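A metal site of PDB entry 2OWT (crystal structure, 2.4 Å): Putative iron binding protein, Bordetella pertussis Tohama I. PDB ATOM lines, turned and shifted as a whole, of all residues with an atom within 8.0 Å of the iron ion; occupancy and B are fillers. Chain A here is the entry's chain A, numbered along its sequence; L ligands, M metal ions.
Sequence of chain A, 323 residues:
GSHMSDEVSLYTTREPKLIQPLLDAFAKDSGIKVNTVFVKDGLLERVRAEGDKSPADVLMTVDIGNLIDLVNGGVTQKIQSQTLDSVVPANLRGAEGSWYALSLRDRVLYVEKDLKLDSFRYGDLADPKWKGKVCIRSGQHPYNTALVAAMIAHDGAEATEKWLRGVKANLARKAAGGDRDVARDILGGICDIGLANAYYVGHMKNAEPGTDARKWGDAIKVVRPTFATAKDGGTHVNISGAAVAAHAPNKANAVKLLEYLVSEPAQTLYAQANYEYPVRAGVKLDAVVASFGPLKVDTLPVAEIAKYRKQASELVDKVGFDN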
ATOM      1  N   THR A  13      23.072 -23.340  -2.878  1.00  0.00           N
ATOM      2  CA  THR A  13      22.528 -23.735  -4.155  1.00  0.00           C
ATOM      3  C   THR A  13      22.979 -22.764  -5.236  1.00  0.00           C
ATOM      4  O   THR A  13      22.603 -22.904  -6.406  1.00  0.00           O
ATOM      5  CB  THR A  13      20.998 -23.763  -4.132  1.00  0.00           C
ATOM      6  OG1 THR A  13      20.529 -22.577  -3.478  1.00  0.00           O
ATOM      7  CG2 THR A  13      20.478 -25.005  -3.411  1.00  0.00           C
ATOM      8  N   ARG A  14      23.788 -21.772  -4.835  1.00  0.00           N
ATOM      9  CA  ARG A  14      24.256 -20.762  -5.771  1.00  0.00           C
ATOM     10  C   ARG A  14      25.198 -21.302  -6.837  1.00  0.00           C
ATOM     11  O   ARG A  14      25.920 -22.279  -6.627  1.00  0.00           O
ATOM     12  CB  ARG A  14      24.885 -19.578  -5.057  1.00  0.00           C
ATOM     13  CG  ARG A  14      23.889 -18.729  -4.269  1.00  0.00           C
ATOM     14  CD  ARG A  14      24.208 -17.253  -4.368  1.00  0.00           C
ATOM     15  NE  ARG A  14      23.947 -16.770  -5.713  1.00  0.00           N
ATOM     16  CZ  ARG A  14      23.848 -15.493  -6.052  1.00  0.00           C
ATOM     17  NH1 ARG A  14      23.996 -14.527  -5.141  1.00  0.00           N
ATOM     18  NH2 ARG A  14      23.601 -15.173  -7.320  1.00  0.00           N
ATOM     19  N   GLU A  15      25.174 -20.659  -7.987  1.00  0.00           N
ATOM     20  CA  GLU A  15      26.179 -20.904  -8.997  1.00  0.00           C
ATOM     21  C   GLU A  15      27.536 -20.468  -8.424  1.00  0.00           C
ATOM     22  O   GLU A  15      27.657 -19.343  -7.890  1.00  0.00           O
ATOM     23  CB  GLU A  15      25.819 -20.118 -10.248  1.00  0.00           C
ATOM     24  CG  GLU A  15      26.010 -20.865 -11.536  1.00  0.00           C
ATOM     25  CD  GLU A  15      25.281 -20.192 -12.681  1.00  0.00           C
ATOM     26  OE1 GLU A  15      25.675 -19.066 -13.029  1.00  0.00           O
ATOM     27  OE2 GLU A  15      24.317 -20.780 -13.214  1.00  0.00           O
ATOM     28  N   LEU A  18      28.948 -17.222  -9.367  1.00  0.00           N
ATOM     29  CA  LEU A  18      28.086 -16.169  -8.813  1.00  0.00           C
ATOM     30  C   LEU A  18      28.230 -15.958  -7.303  1.00  0.00           C
ATOM     31  O   LEU A  18      27.538 -15.121  -6.715  1.00  0.00           O
ATOM     32  CB  LEU A  18      26.610 -16.437  -9.167  1.00  0.00           C
ATOM     33  CG  LEU A  18      26.252 -16.298 -10.650  1.00  0.00           C
ATOM     34  CD1 LEU A  18      24.792 -16.595 -10.859  1.00  0.00           C
ATOM     35  CD2 LEU A  18      26.614 -14.905 -11.190  1.00  0.00           C
ATOM     36  N   VAL A  62      18.973 -19.270  -3.189  1.00  0.00           N
ATOM     37  CA  VAL A  62      18.568 -18.238  -4.136  1.00  0.00           C
ATOM     38  C   VAL A  62      17.042 -18.203  -4.277  1.00  0.00           C
ATOM     39  O   VAL A  62      16.507 -17.970  -5.367  1.00  0.00           O
ATOM     40  CB  VAL A  62      19.245 -18.428  -5.511  1.00  0.00           C
ATOM     41  CG1 VAL A  62      20.628 -17.784  -5.506  1.00  0.00           C
ATOM     42  CG2 VAL A  62      19.302 -19.911  -5.912  1.00  0.00           C
ATOM     43  N   ARG A 105      16.568  -9.962  -6.773  1.00  0.00           N
ATOM     44  CA  ARG A 105      16.494 -10.362  -8.168  1.00  0.00           C
ATOM     45  C   ARG A 105      15.035 -10.326  -8.602  1.00  0.00           C
ATOM     46  O   ARG A 105      14.144 -10.505  -7.776  1.00  0.00           O
ATOM     47  CB  ARG A 105      17.019 -11.783  -8.362  1.00  0.00           C
ATOM     48  CG  ARG A 105      16.648 -12.748  -7.235  1.00  0.00           C
ATOM     49  CD  ARG A 105      17.893 -13.264  -6.529  1.00  0.00           C
ATOM     50  NE  ARG A 105      18.094 -14.606  -7.044  1.00  0.00           N
ATOM     51  CZ  ARG A 105      19.239 -15.138  -7.413  1.00  0.00           C
ATOM     52  NH1 ARG A 105      20.380 -14.477  -7.313  1.00  0.00           N
ATOM     53  NH2 ARG A 105      19.219 -16.361  -7.893  1.00  0.00           N
ATOM     54  N   ARG A 107      12.113 -11.769 -11.599  1.00  0.00           N
ATOM     55  CA  ARG A 107      11.799 -12.700 -12.675  1.00  0.00           C
ATOM     56  C   ARG A 107      11.037 -11.930 -13.731  1.00  0.00           C
ATOM     57  O   ARG A 107       9.932 -11.453 -13.488  1.00  0.00           O
ATOM     58  CB  ARG A 107      10.994 -13.889 -12.153  1.00  0.00           C
ATOM     59  CG  ARG A 107      11.031 -15.107 -13.066  1.00  0.00           C
ATOM     60  CD  ARG A 107      10.969 -16.397 -12.278  1.00  0.00           C
ATOM     61  NE  ARG A 107      11.263 -17.573 -13.093  1.00  0.00           N
ATOM     62  CZ  ARG A 107      12.470 -17.921 -13.542  1.00  0.00           C
ATOM     63  NH1 ARG A 107      13.533 -17.163 -13.275  1.00  0.00           N
ATOM     64  NH2 ARG A 107      12.615 -19.028 -14.258  1.00  0.00           N
ATOM     65  N   ARG A 137      12.188 -22.574 -18.068  1.00  0.00           N
ATOM     66  CA  ARG A 137      12.789 -23.755 -17.425  1.00  0.00           C
ATOM     67  C   ARG A 137      11.699 -24.538 -16.675  1.00  0.00           C
ATOM     68  O   ARG A 137      10.542 -24.114 -16.664  1.00  0.00           O
ATOM     69  CB  ARG A 137      13.924 -23.361 -16.490  1.00  0.00           C
ATOM     70  CG  ARG A 137      13.496 -22.801 -15.127  1.00  0.00           C
ATOM     71  CD  ARG A 137      14.697 -22.268 -14.336  1.00  0.00           C
ATOM     72  NE  ARG A 137      15.765 -23.272 -14.141  1.00  0.00           N
ATOM     73  CZ  ARG A 137      16.944 -23.005 -13.604  1.00  0.00           C
ATOM     74  NH1 ARG A 137      17.247 -21.770 -13.201  1.00  0.00           N
ATOM     75  NH2 ARG A 137      17.860 -23.965 -13.478  1.00  0.00           N
ATOM     76  N   HIS A 141      11.346 -25.649 -10.574  1.00  0.00           N
ATOM     77  CA  HIS A 141      12.517 -24.918 -10.082  1.00  0.00           C
ATOM     78  C   HIS A 141      12.062 -23.785  -9.150  1.00  0.00           C
ATOM     79  O   HIS A 141      11.054 -23.138  -9.432  1.00  0.00           O
ATOM     80  CB  HIS A 141      13.386 -24.355 -11.215  1.00  0.00           C
ATOM     81  CG  HIS A 141      14.703 -23.827 -10.739  1.00  0.00           C
ATOM     82  ND1 HIS A 141      14.853 -22.536 -10.277  1.00  0.00           N
ATOM     83  CD2 HIS A 141      15.898 -24.436 -10.561  1.00  0.00           C
ATOM     84  CE1 HIS A 141      16.095 -22.368  -9.863  1.00  0.00           C
ATOM     85  NE2 HIS A 141      16.755 -23.500 -10.022  1.00  0.00           N
ATOM     86  N   TYR A 143      12.833 -20.698  -8.584  1.00  0.00           N
ATOM     87  CA  TYR A 143      12.530 -19.394  -9.188  1.00  0.00           C
ATOM     88  C   TYR A 143      11.071 -19.329  -9.632  1.00  0.00           C
ATOM     89  O   TYR A 143      10.408 -18.304  -9.444  1.00  0.00           O
ATOM     90  CB  TYR A 143      13.441 -19.089 -10.403  1.00  0.00           C
ATOM     91  CG  TYR A 143      14.940 -19.030 -10.143  1.00  0.00           C
ATOM     92  CD1 TYR A 143      15.848 -19.277 -11.169  1.00  0.00           C
ATOM     93  CD2 TYR A 143      15.445 -18.718  -8.889  1.00  0.00           C
ATOM     94  CE1 TYR A 143      17.212 -19.226 -10.943  1.00  0.00           C
ATOM     95  CE2 TYR A 143      16.811 -18.673  -8.650  1.00  0.00           C
ATOM     96  CZ  TYR A 143      17.683 -18.923  -9.676  1.00  0.00           C
ATOM     97  OH  TYR A 143      19.041 -18.868  -9.437  1.00  0.00           O
ATOM     98  N   ASP A 179      17.863 -20.806 -16.842  1.00  0.00           N
ATOM     99  CA  ASP A 179      17.340 -19.490 -17.228  1.00  0.00           C
ATOM    100  C   ASP A 179      18.027 -18.932 -18.494  1.00  0.00           C
ATOM    101  O   ASP A 179      17.370 -18.259 -19.301  1.00  0.00           O
ATOM    102  CB  ASP A 179      17.466 -18.496 -16.071  1.00  0.00           C
ATOM    103  CG  ASP A 179      16.206 -18.424 -15.210  1.00  0.00           C
ATOM    104  OD1 ASP A 179      15.293 -19.246 -15.394  1.00  0.00           O
ATOM    105  OD2 ASP A 179      16.128 -17.508 -14.355  1.00  0.00           O
ATOM    106  N   ARG A 180      19.320 -19.221 -18.669  1.00  0.00           N
ATOM    107  CA  ARG A 180      20.088 -18.758 -19.825  1.00  0.00           C
ATOM    108  C   ARG A 180      19.602 -19.349 -21.149  1.00  0.00           C
ATOM    109  O   ARG A 180      19.609 -18.693 -22.188  1.00  0.00           O
ATOM    110  CB  ARG A 180      21.608 -18.975 -19.618  1.00  0.00           C
ATOM    111  CG  ARG A 180      22.300 -17.784 -18.950  1.00  0.00           C
ATOM    112  CD  ARG A 180      23.761 -18.083 -18.533  1.00  0.00           C
ATOM    113  NE  ARG A 180      23.755 -18.940 -17.368  1.00  0.00           N
ATOM    114  CZ  ARG A 180      24.326 -18.704 -16.193  1.00  0.00           C
ATOM    115  NH1 ARG A 180      25.066 -17.619 -15.963  1.00  0.00           N
ATOM    116  NH2 ARG A 180      24.177 -19.612 -15.241  1.00  0.00           N
ATOM    117  N   ASN A 197      15.305 -14.802 -14.881  1.00  0.00           N
ATOM    118  CA  ASN A 197      15.874 -13.768 -13.999  1.00  0.00           C
ATOM    119  C   ASN A 197      16.730 -12.778 -14.779  1.00  0.00           C
ATOM    120  O   ASN A 197      17.573 -13.159 -15.603  1.00  0.00           O
ATOM    121  CB  ASN A 197      16.663 -14.405 -12.844  1.00  0.00           C
ATOM    122  CG  ASN A 197      15.751 -15.066 -11.772  1.00  0.00           C
ATOM    123  OD1 ASN A 197      14.542 -14.858 -11.749  1.00  0.00           O
ATOM    124  ND2 ASN A 197      16.344 -15.860 -10.919  1.00  0.00           N
ATOM    125  N   TYR A 199      19.158 -10.783 -13.909  1.00  0.00           N
ATOM    126  CA  TYR A 199      20.594 -10.733 -13.645  1.00  0.00           C
ATOM    127  C   TYR A 199      21.418 -11.580 -14.622  1.00  0.00           C
ATOM    128  O   TYR A 199      22.556 -11.230 -14.926  1.00  0.00           O
ATOM    129  CB  TYR A 199      20.932 -11.041 -12.167  1.00  0.00           C
ATOM    130  CG  TYR A 199      20.571 -12.415 -11.684  1.00  0.00           C
ATOM    131  CD1 TYR A 199      21.441 -13.495 -11.880  1.00  0.00           C
ATOM    132  CD2 TYR A 199      19.389 -12.650 -11.003  1.00  0.00           C
ATOM    133  CE1 TYR A 199      21.113 -14.767 -11.435  1.00  0.00           C
ATOM    134  CE2 TYR A 199      19.052 -13.912 -10.559  1.00  0.00           C
ATOM    135  CZ  TYR A 199      19.914 -14.970 -10.775  1.00  0.00           C
ATOM    136  OH  TYR A 199      19.582 -16.227 -10.338  1.00  0.00           O
ATOM    137  N   TYR A 200      20.847 -12.678 -15.122  1.00  0.00           N
ATOM    138  CA  TYR A 200      21.505 -13.503 -16.149  1.00  0.00           C
ATOM    139  C   TYR A 200      21.699 -12.731 -17.463  1.00  0.00           C
ATOM    140  O   TYR A 200      22.730 -12.902 -18.111  1.00  0.00           O
ATOM    141  CB  TYR A 200      20.756 -14.807 -16.420  1.00  0.00           C
ATOM    142  CG  TYR A 200      20.756 -15.791 -15.270  1.00  0.00           C
ATOM    143  CD1 TYR A 200      19.579 -16.086 -14.581  1.00  0.00           C
ATOM    144  CD2 TYR A 200      21.930 -16.438 -14.870  1.00  0.00           C
ATOM    145  CE1 TYR A 200      19.570 -16.989 -13.526  1.00  0.00           C
ATOM    146  CE2 TYR A 200      21.930 -17.343 -13.810  1.00  0.00           C
ATOM    147  CZ  TYR A 200      20.745 -17.617 -13.140  1.00  0.00           C
ATOM    148  OH  TYR A 200      20.737 -18.528 -12.090  1.00  0.00           O
ATOM    149  N   SER A 240      18.535 -13.729  -2.825  1.00  0.00           N
ATOM    150  CA  SER A 240      19.489 -14.680  -2.339  1.00  0.00           C
ATOM    151  C   SER A 240      19.519 -14.381  -0.845  1.00  0.00           C
ATOM    152  O   SER A 240      19.391 -13.214  -0.436  1.00  0.00           O
ATOM    153  CB  SER A 240      20.864 -14.531  -3.015  1.00  0.00           C
ATOM    154  OG  SER A 240      21.735 -13.651  -2.322  1.00  0.00           O
ATOM    155  N   GLU A 276      22.906  -8.245  -9.946  1.00  0.00           N
ATOM    156  CA  GLU A 276      21.729  -8.280  -9.103  1.00  0.00           C
ATOM    157  C   GLU A 276      21.467  -6.895  -8.510  1.00  0.00           C
ATOM    158  O   GLU A 276      22.137  -5.921  -8.860  1.00  0.00           O
ATOM    159  CB  GLU A 276      21.916  -9.298  -7.963  1.00  0.00           C
ATOM    160  CG  GLU A 276      21.894 -10.739  -8.395  1.00  0.00           C
ATOM    161  CD  GLU A 276      22.159 -11.689  -7.241  1.00  0.00           C
ATOM    162  OE1 GLU A 276      23.333 -12.079  -7.030  1.00  0.00           O
ATOM    163  OE2 GLU A 276      21.206 -12.031  -6.528  1.00  0.00           O
HETATM  164  C1  LIG L   1      22.438 -18.321  -8.842  1.00  0.00           C
HETATM  165  O1  LIG L   1      22.179 -19.342  -9.605  1.00  0.00           O
HETATM  166  O2  LIG L   1      21.753 -17.234  -9.016  1.00  0.00           O
HETATM  167  O3  LIG L   1      23.354 -18.376  -7.934  1.00  0.00           O
HETATM  168 FE    FE M   1      20.427 -17.911 -10.227  1.00  0.00          FE
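NH2 of Arg 105 sits close to OH of Tyr 143 (2.9 Å).
N of Tyr 143 lies within hydrogen-bond range of ND1 of His 141 (3.2 Å).
The side-chain hydroxyl of Tyr 199 sits close to the guanidinium group of Arg 105 (2.5 Å).
OH of Tyr 199 lies close to ND2 of Asn 197, 3.3 Å away.
The guanidinium group (NH1) of Arg 105 is in salt-bridge range of the side-chain carboxylate (OE2) of Glu 276, 2.7 Å away.
Residues that only touch the iron ion: Arg 105 (3.1 Å).
Four residues have an atom within 4 Å of the iron ion: Arg 105, Tyr 143, Tyr 199 and Tyr 200.
The nearest printed residue that does not touch the iron ion is Leu 18 (4.6 Å).
OH of Tyr 143 binds the iron ion (1.9 Å).
The iron ion is bound by OH of Tyr 199 (1.9 Å).
An oxygen (O2) of the ligand binds the iron ion, 1.9 Å away.
The iron ion is bound by the side-chain hydroxyl (OH) of Tyr 200.
An oxygen (O1) of the ligand is bound to the iron ion.
The iron ion has five donor atoms within binding distance.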
